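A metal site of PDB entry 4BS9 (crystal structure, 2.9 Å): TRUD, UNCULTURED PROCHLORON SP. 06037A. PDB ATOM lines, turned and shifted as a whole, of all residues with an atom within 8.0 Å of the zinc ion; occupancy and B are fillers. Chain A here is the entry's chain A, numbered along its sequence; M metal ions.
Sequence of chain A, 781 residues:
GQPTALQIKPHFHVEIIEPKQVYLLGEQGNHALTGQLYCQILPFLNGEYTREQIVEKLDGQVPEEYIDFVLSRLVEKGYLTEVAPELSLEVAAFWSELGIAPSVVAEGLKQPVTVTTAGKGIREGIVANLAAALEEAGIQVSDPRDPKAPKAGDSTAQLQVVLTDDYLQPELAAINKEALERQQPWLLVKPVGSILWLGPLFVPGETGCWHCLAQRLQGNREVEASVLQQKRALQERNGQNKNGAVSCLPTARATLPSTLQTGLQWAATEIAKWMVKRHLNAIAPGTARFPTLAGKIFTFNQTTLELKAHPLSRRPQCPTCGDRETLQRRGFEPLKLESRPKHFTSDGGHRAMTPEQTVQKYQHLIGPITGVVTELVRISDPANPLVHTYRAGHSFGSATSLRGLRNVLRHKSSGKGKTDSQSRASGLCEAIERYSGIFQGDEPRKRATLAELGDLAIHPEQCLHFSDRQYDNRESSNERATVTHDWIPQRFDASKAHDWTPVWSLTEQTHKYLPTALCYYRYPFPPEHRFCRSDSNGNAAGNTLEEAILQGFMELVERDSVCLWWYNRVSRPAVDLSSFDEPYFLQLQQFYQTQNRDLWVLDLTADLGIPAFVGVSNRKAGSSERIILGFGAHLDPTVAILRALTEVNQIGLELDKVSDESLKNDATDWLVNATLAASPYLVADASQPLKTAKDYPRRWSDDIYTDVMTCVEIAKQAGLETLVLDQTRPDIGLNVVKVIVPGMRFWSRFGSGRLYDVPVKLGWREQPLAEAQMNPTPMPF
Four residues have an atom within 4 Å of the zinc ion: Cys 209, Cys 212, Cys 318 and Cys 321.
N of His 211 lies close to SG of Cys 209, at 3.3 Å. SG of Cys 209 sits close to ND2 of Asn 176, at 3.5 Å. The side-chain sulfur of Cys 212 sits close to the backbone NH of Arg 315, 3.5 Å away. The backbone NH of Thr 320 lies close to the side-chain sulfur of Cys 318 (3.4 Å). NH2 of Arg 314 sits at hydrogen-bond distance from O of Cys 321, 3.5 Å away.
The zinc ion is bound by SG of Cys 209, 2.4 Å away. SG of Cys 212 binds the zinc ion, 2.4 Å away. The zinc ion is bound by the side-chain sulfur (SG) of Cys 318 (2.4 Å). The zinc ion is bound by SG of Cys 321 (2.4 Å). The zinc ion has four donor atoms within binding distance.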
ATOM      1  N   ASN A 176      24.353  12.366  26.599  1.00  0.00           N
ATOM      2  CA  ASN A 176      23.223  12.896  27.350  1.00  0.00           C
ATOM      3  C   ASN A 176      23.552  13.117  28.843  1.00  0.00           C
ATOM      4  O   ASN A 176      23.134  14.123  29.416  1.00  0.00           O
ATOM      5  CB  ASN A 176      22.059  11.918  27.212  1.00  0.00           C
ATOM      6  CG  ASN A 176      20.759  12.486  27.723  1.00  0.00           C
ATOM      7  OD1 ASN A 176      20.289  13.494  27.229  1.00  0.00           O
ATOM      8  ND2 ASN A 176      20.160  11.806  28.683  1.00  0.00           N
ATOM      9  N   LEU A 180      23.882  16.644  30.727  1.00  0.00           N
ATOM     10  CA  LEU A 180      23.042  16.949  31.871  1.00  0.00           C
ATOM     11  C   LEU A 180      23.878  17.443  33.017  1.00  0.00           C
ATOM     12  O   LEU A 180      23.528  18.475  33.587  1.00  0.00           O
ATOM     13  CB  LEU A 180      22.136  15.786  32.293  1.00  0.00           C
ATOM     14  CG  LEU A 180      20.949  15.637  31.325  1.00  0.00           C
ATOM     15  CD1 LEU A 180      20.085  14.445  31.681  1.00  0.00           C
ATOM     16  CD2 LEU A 180      20.093  16.895  31.265  1.00  0.00           C
ATOM     17  N   PHE A 202      18.668  19.818  22.535  1.00  0.00           N
ATOM     18  CA  PHE A 202      18.433  19.566  23.934  1.00  0.00           C
ATOM     19  C   PHE A 202      19.052  20.697  24.758  1.00  0.00           C
ATOM     20  O   PHE A 202      20.199  21.062  24.519  1.00  0.00           O
ATOM     21  CB  PHE A 202      19.086  18.259  24.363  1.00  0.00           C
ATOM     22  CG  PHE A 202      18.633  17.053  23.588  1.00  0.00           C
ATOM     23  CD1 PHE A 202      17.507  16.361  23.962  1.00  0.00           C
ATOM     24  CD2 PHE A 202      19.392  16.567  22.529  1.00  0.00           C
ATOM     25  CE1 PHE A 202      17.109  15.232  23.254  1.00  0.00           C
ATOM     26  CE2 PHE A 202      19.003  15.438  21.819  1.00  0.00           C
ATOM     27  CZ  PHE A 202      17.864  14.764  22.183  1.00  0.00           C
ATOM     28  N   THR A 207      14.308  21.464  28.118  1.00  0.00           N
ATOM     29  CA  THR A 207      13.730  20.466  27.229  1.00  0.00           C
ATOM     30  C   THR A 207      13.757  19.076  27.865  1.00  0.00           C
ATOM     31  O   THR A 207      14.131  18.912  29.029  1.00  0.00           O
ATOM     32  CB  THR A 207      14.554  20.361  25.946  1.00  0.00           C
ATOM     33  OG1 THR A 207      15.834  19.794  26.262  1.00  0.00           O
ATOM     34  CG2 THR A 207      14.700  21.715  25.275  1.00  0.00           C
ATOM     35  N   GLY A 208      13.356  18.075  27.079  1.00  0.00           N
ATOM     36  CA  GLY A 208      13.560  16.665  27.421  1.00  0.00           C
ATOM     37  C   GLY A 208      15.014  16.289  27.271  1.00  0.00           C
ATOM     38  O   GLY A 208      15.809  17.042  26.694  1.00  0.00           O
ATOM     39  N   CYS A 209      15.391  15.143  27.817  1.00  0.00           N
ATOM     40  CA  CYS A 209      16.734  14.639  27.549  1.00  0.00           C
ATOM     41  C   CYS A 209      16.619  13.662  26.380  1.00  0.00           C
ATOM     42  O   CYS A 209      15.520  13.389  25.890  1.00  0.00           O
ATOM     43  CB  CYS A 209      17.334  14.014  28.802  1.00  0.00           C
ATOM     44  SG  CYS A 209      16.735  12.370  29.096  1.00  0.00           S
ATOM     45  N   TRP A 210      17.758  13.142  25.922  1.00  0.00           N
ATOM     46  CA  TRP A 210      17.760  12.143  24.850  1.00  0.00           C
ATOM     47  C   TRP A 210      17.010  10.878  25.211  1.00  0.00           C
ATOM     48  O   TRP A 210      16.366  10.258  24.354  1.00  0.00           O
ATOM     49  CB  TRP A 210      19.182  11.760  24.499  1.00  0.00           C
ATOM     50  CG  TRP A 210      19.250  10.553  23.654  1.00  0.00           C
ATOM     51  CD1 TRP A 210      19.126  10.492  22.305  1.00  0.00           C
ATOM     52  CD2 TRP A 210      19.418   9.214  24.111  1.00  0.00           C
ATOM     53  NE1 TRP A 210      19.226   9.191  21.888  1.00  0.00           N
ATOM     54  CE2 TRP A 210      19.406   8.386  22.988  1.00  0.00           C
ATOM     55  CE3 TRP A 210      19.581   8.628  25.371  1.00  0.00           C
ATOM     56  CZ2 TRP A 210      19.560   7.009  23.064  1.00  0.00           C
ATOM     57  CZ3 TRP A 210      19.735   7.268  25.457  1.00  0.00           C
ATOM     58  CH2 TRP A 210      19.715   6.471  24.320  1.00  0.00           C
ATOM     59  N   HIS A 211      17.128  10.475  26.476  1.00  0.00           N
ATOM     60  CA  HIS A 211      16.336   9.363  27.027  1.00  0.00           C
ATOM     61  C   HIS A 211      14.813   9.615  27.015  1.00  0.00           C
ATOM     62  O   HIS A 211      14.020   8.652  26.934  1.00  0.00           O
ATOM     63  CB  HIS A 211      16.837   9.012  28.426  1.00  0.00           C
ATOM     64  CG  HIS A 211      16.288   7.723  28.944  1.00  0.00           C
ATOM     65  ND1 HIS A 211      16.426   7.345  30.265  1.00  0.00           N
ATOM     66  CD2 HIS A 211      15.561   6.749  28.342  1.00  0.00           C
ATOM     67  CE1 HIS A 211      15.809   6.188  30.449  1.00  0.00           C
ATOM     68  NE2 HIS A 211      15.284   5.809  29.291  1.00  0.00           N
ATOM     69  N   CYS A 212      14.384  10.867  27.066  1.00  0.00           N
ATOM     70  CA  CYS A 212      12.946  11.148  26.890  1.00  0.00           C
ATOM     71  C   CYS A 212      12.524  10.713  25.499  1.00  0.00           C
ATOM     72  O   CYS A 212      11.489  10.062  25.305  1.00  0.00           O
ATOM     73  CB  CYS A 212      12.653  12.640  27.106  1.00  0.00           C
ATOM     74  SG  CYS A 212      12.875  13.158  28.822  1.00  0.00           S
ATOM     75  N   LEU A 213      13.376  11.064  24.544  1.00  0.00           N
ATOM     76  CA  LEU A 213      13.198  10.717  23.146  1.00  0.00           C
ATOM     77  C   LEU A 213      13.288   9.188  22.969  1.00  0.00           C
ATOM     78  O   LEU A 213      12.396   8.567  22.400  1.00  0.00           O
ATOM     79  CB  LEU A 213      14.263  11.431  22.310  1.00  0.00           C
ATOM     80  CG  LEU A 213      14.416  10.936  20.870  1.00  0.00           C
ATOM     81  CD1 LEU A 213      13.300  11.487  20.003  1.00  0.00           C
ATOM     82  CD2 LEU A 213      15.770  11.341  20.316  1.00  0.00           C
ATOM     83  N   ALA A 214      14.347   8.599  23.493  1.00  0.00           N
ATOM     84  CA  ALA A 214      14.622   7.202  23.256  1.00  0.00           C
ATOM     85  C   ALA A 214      13.567   6.216  23.768  1.00  0.00           C
ATOM     86  O   ALA A 214      13.303   5.255  23.074  1.00  0.00           O
ATOM     87  CB  ALA A 214      15.997   6.841  23.812  1.00  0.00           C
ATOM     88  N   LEU A 312       9.381  16.934  20.857  1.00  0.00           N
ATOM     89  CA  LEU A 312       9.854  16.139  21.984  1.00  0.00           C
ATOM     90  C   LEU A 312       9.192  16.566  23.317  1.00  0.00           C
ATOM     91  O   LEU A 312       9.316  17.697  23.709  1.00  0.00           O
ATOM     92  CB  LEU A 312      11.381  16.253  22.107  1.00  0.00           C
ATOM     93  CG  LEU A 312      11.993  15.633  23.371  1.00  0.00           C
ATOM     94  CD1 LEU A 312      11.685  14.148  23.483  1.00  0.00           C
ATOM     95  CD2 LEU A 312      13.490  15.875  23.436  1.00  0.00           C
ATOM     96  N   SER A 313       8.539  15.646  24.015  1.00  0.00           N
ATOM     97  CA  SER A 313       7.958  15.908  25.333  1.00  0.00           C
ATOM     98  C   SER A 313       8.966  15.543  26.393  1.00  0.00           C
ATOM     99  O   SER A 313       9.632  14.506  26.281  1.00  0.00           O
ATOM    100  CB  SER A 313       6.715  15.047  25.579  1.00  0.00           C
ATOM    101  OG  SER A 313       5.629  15.452  24.759  1.00  0.00           O
ATOM    102  N   ARG A 314       9.066  16.362  27.435  1.00  0.00           N
ATOM    103  CA  ARG A 314       9.945  16.071  28.566  1.00  0.00           C
ATOM    104  C   ARG A 314       9.155  15.227  29.543  1.00  0.00           C
ATOM    105  O   ARG A 314       8.135  15.659  30.070  1.00  0.00           O
ATOM    106  CB  ARG A 314      10.407  17.360  29.243  1.00  0.00           C
ATOM    107  CG  ARG A 314      11.434  17.131  30.330  1.00  0.00           C
ATOM    108  CD  ARG A 314      11.236  18.027  31.532  1.00  0.00           C
ATOM    109  NE  ARG A 314      12.261  17.790  32.555  1.00  0.00           N
ATOM    110  CZ  ARG A 314      13.226  18.645  32.894  1.00  0.00           C
ATOM    111  NH1 ARG A 314      13.317  19.829  32.292  1.00  0.00           N
ATOM    112  NH2 ARG A 314      14.104  18.312  33.843  1.00  0.00           N
ATOM    113  N   ARG A 315       9.620  14.011  29.781  1.00  0.00           N
ATOM    114  CA  ARG A 315       8.851  13.029  30.524  1.00  0.00           C
ATOM    115  C   ARG A 315       9.061  13.204  32.013  1.00  0.00           C
ATOM    116  O   ARG A 315      10.149  12.961  32.508  1.00  0.00           O
ATOM    117  CB  ARG A 315       9.262  11.612  30.090  1.00  0.00           C
ATOM    118  CG  ARG A 315       8.786  11.260  28.694  1.00  0.00           C
ATOM    119  CD  ARG A 315       9.110   9.819  28.319  1.00  0.00           C
ATOM    120  NE  ARG A 315       8.239   8.833  28.970  1.00  0.00           N
ATOM    121  CZ  ARG A 315       8.643   7.896  29.827  1.00  0.00           C
ATOM    122  NH1 ARG A 315       9.920   7.779  30.174  1.00  0.00           N
ATOM    123  NH2 ARG A 315       7.772   7.030  30.358  1.00  0.00           N
ATOM    124  N   PRO A 316       8.017  13.606  32.745  1.00  0.00           N
ATOM    125  CA  PRO A 316       8.200  13.824  34.184  1.00  0.00           C
ATOM    126  C   PRO A 316       8.892  12.681  34.904  1.00  0.00           C
ATOM    127  O   PRO A 316       9.654  12.932  35.830  1.00  0.00           O
ATOM    128  CB  PRO A 316       6.787  14.009  34.689  1.00  0.00           C
ATOM    129  CG  PRO A 316       6.048  14.603  33.543  1.00  0.00           C
ATOM    130  CD  PRO A 316       6.668  14.018  32.297  1.00  0.00           C
ATOM    131  N   GLN A 317       8.650  11.453  34.476  1.00  0.00           N
ATOM    132  CA  GLN A 317       9.170  10.285  35.196  1.00  0.00           C
ATOM    133  C   GLN A 317      10.434   9.710  34.560  1.00  0.00           C
ATOM    134  O   GLN A 317      10.794   8.552  34.779  1.00  0.00           O
ATOM    135  CB  GLN A 317       8.087   9.209  35.277  1.00  0.00           C
ATOM    136  CG  GLN A 317       7.795   8.534  33.956  1.00  0.00           C
ATOM    137  CD  GLN A 317       6.764   9.272  33.128  1.00  0.00           C
ATOM    138  OE1 GLN A 317       6.884  10.473  32.865  1.00  0.00           O
ATOM    139  NE2 GLN A 317       5.725   8.541  32.718  1.00  0.00           N
ATOM    140  N   CYS A 318      11.086  10.519  33.734  1.00  0.00           N
ATOM    141  CA  CYS A 318      12.216  10.040  33.015  1.00  0.00           C
ATOM    142  C   CYS A 318      13.242   9.590  34.006  1.00  0.00           C
ATOM    143  O   CYS A 318      13.662  10.376  34.837  1.00  0.00           O
ATOM    144  CB  CYS A 318      12.790  11.155  32.168  1.00  0.00           C
ATOM    145  SG  CYS A 318      14.328  10.608  31.432  1.00  0.00           S
ATOM    146  N   PRO A 319      13.642   8.317  33.951  1.00  0.00           N
ATOM    147  CA  PRO A 319      14.688   7.830  34.866  1.00  0.00           C
ATOM    148  C   PRO A 319      15.972   8.661  34.843  1.00  0.00           C
ATOM    149  O   PRO A 319      16.588   8.850  35.871  1.00  0.00           O
ATOM    150  CB  PRO A 319      14.964   6.411  34.375  1.00  0.00           C
ATOM    151  CG  PRO A 319      13.769   6.017  33.599  1.00  0.00           C
ATOM    152  CD  PRO A 319      13.178   7.267  33.034  1.00  0.00           C
ATOM    153  N   THR A 320      16.369   9.146  33.681  1.00  0.00           N
ATOM    154  CA  THR A 320      17.591   9.941  33.582  1.00  0.00           C
ATOM    155  C   THR A 320      17.431  11.401  34.064  1.00  0.00           C
ATOM    156  O   THR A 320      18.203  11.838  34.918  1.00  0.00           O
ATOM    157  CB  THR A 320      18.165   9.916  32.144  1.00  0.00           C
ATOM    158  OG1 THR A 320      18.500   8.577  31.792  1.00  0.00           O
ATOM    159  CG2 THR A 320      19.403  10.744  32.049  1.00  0.00           C
ATOM    160  N   CYS A 321      16.463  12.138  33.530  1.00  0.00           N
ATOM    161  CA  CYS A 321      16.352  13.553  33.874  1.00  0.00           C
ATOM    162  C   CYS A 321      15.104  13.923  34.695  1.00  0.00           C
ATOM    163  O   CYS A 321      14.828  15.103  34.885  1.00  0.00           O
ATOM    164  CB  CYS A 321      16.400  14.391  32.606  1.00  0.00           C
ATOM    165  SG  CYS A 321      14.819  14.529  31.759  1.00  0.00           S
ATOM    166  N   GLY A 322      14.391  12.936  35.214  1.00  0.00           N
ATOM    167  CA  GLY A 322      13.166  13.183  35.966  1.00  0.00           C
ATOM    168  C   GLY A 322      13.083  12.385  37.244  1.00  0.00           C
ATOM    169  O   GLY A 322      14.108  12.148  37.882  1.00  0.00           O
ATOM    170  N   ASP A 323      11.868  12.007  37.641  1.00  0.00           N
ATOM    171  CA  ASP A 323      11.638  11.228  38.865  1.00  0.00           C
ATOM    172  C   ASP A 323      11.145   9.808  38.540  1.00  0.00           C
ATOM    173  O   ASP A 323       9.965   9.584  38.236  1.00  0.00           O
ATOM    174  CB  ASP A 323      10.649  11.954  39.776  1.00  0.00           C
ATOM    175  CG  ASP A 323      10.473  11.257  41.119  1.00  0.00           C
ATOM    176  OD1 ASP A 323      11.177  10.268  41.410  1.00  0.00           O
ATOM    177  OD2 ASP A 323       9.603  11.730  41.890  1.00  0.00           O
HETATM  178 ZN    ZN M   1      14.697  12.658  30.270  1.00  0.00          ZN
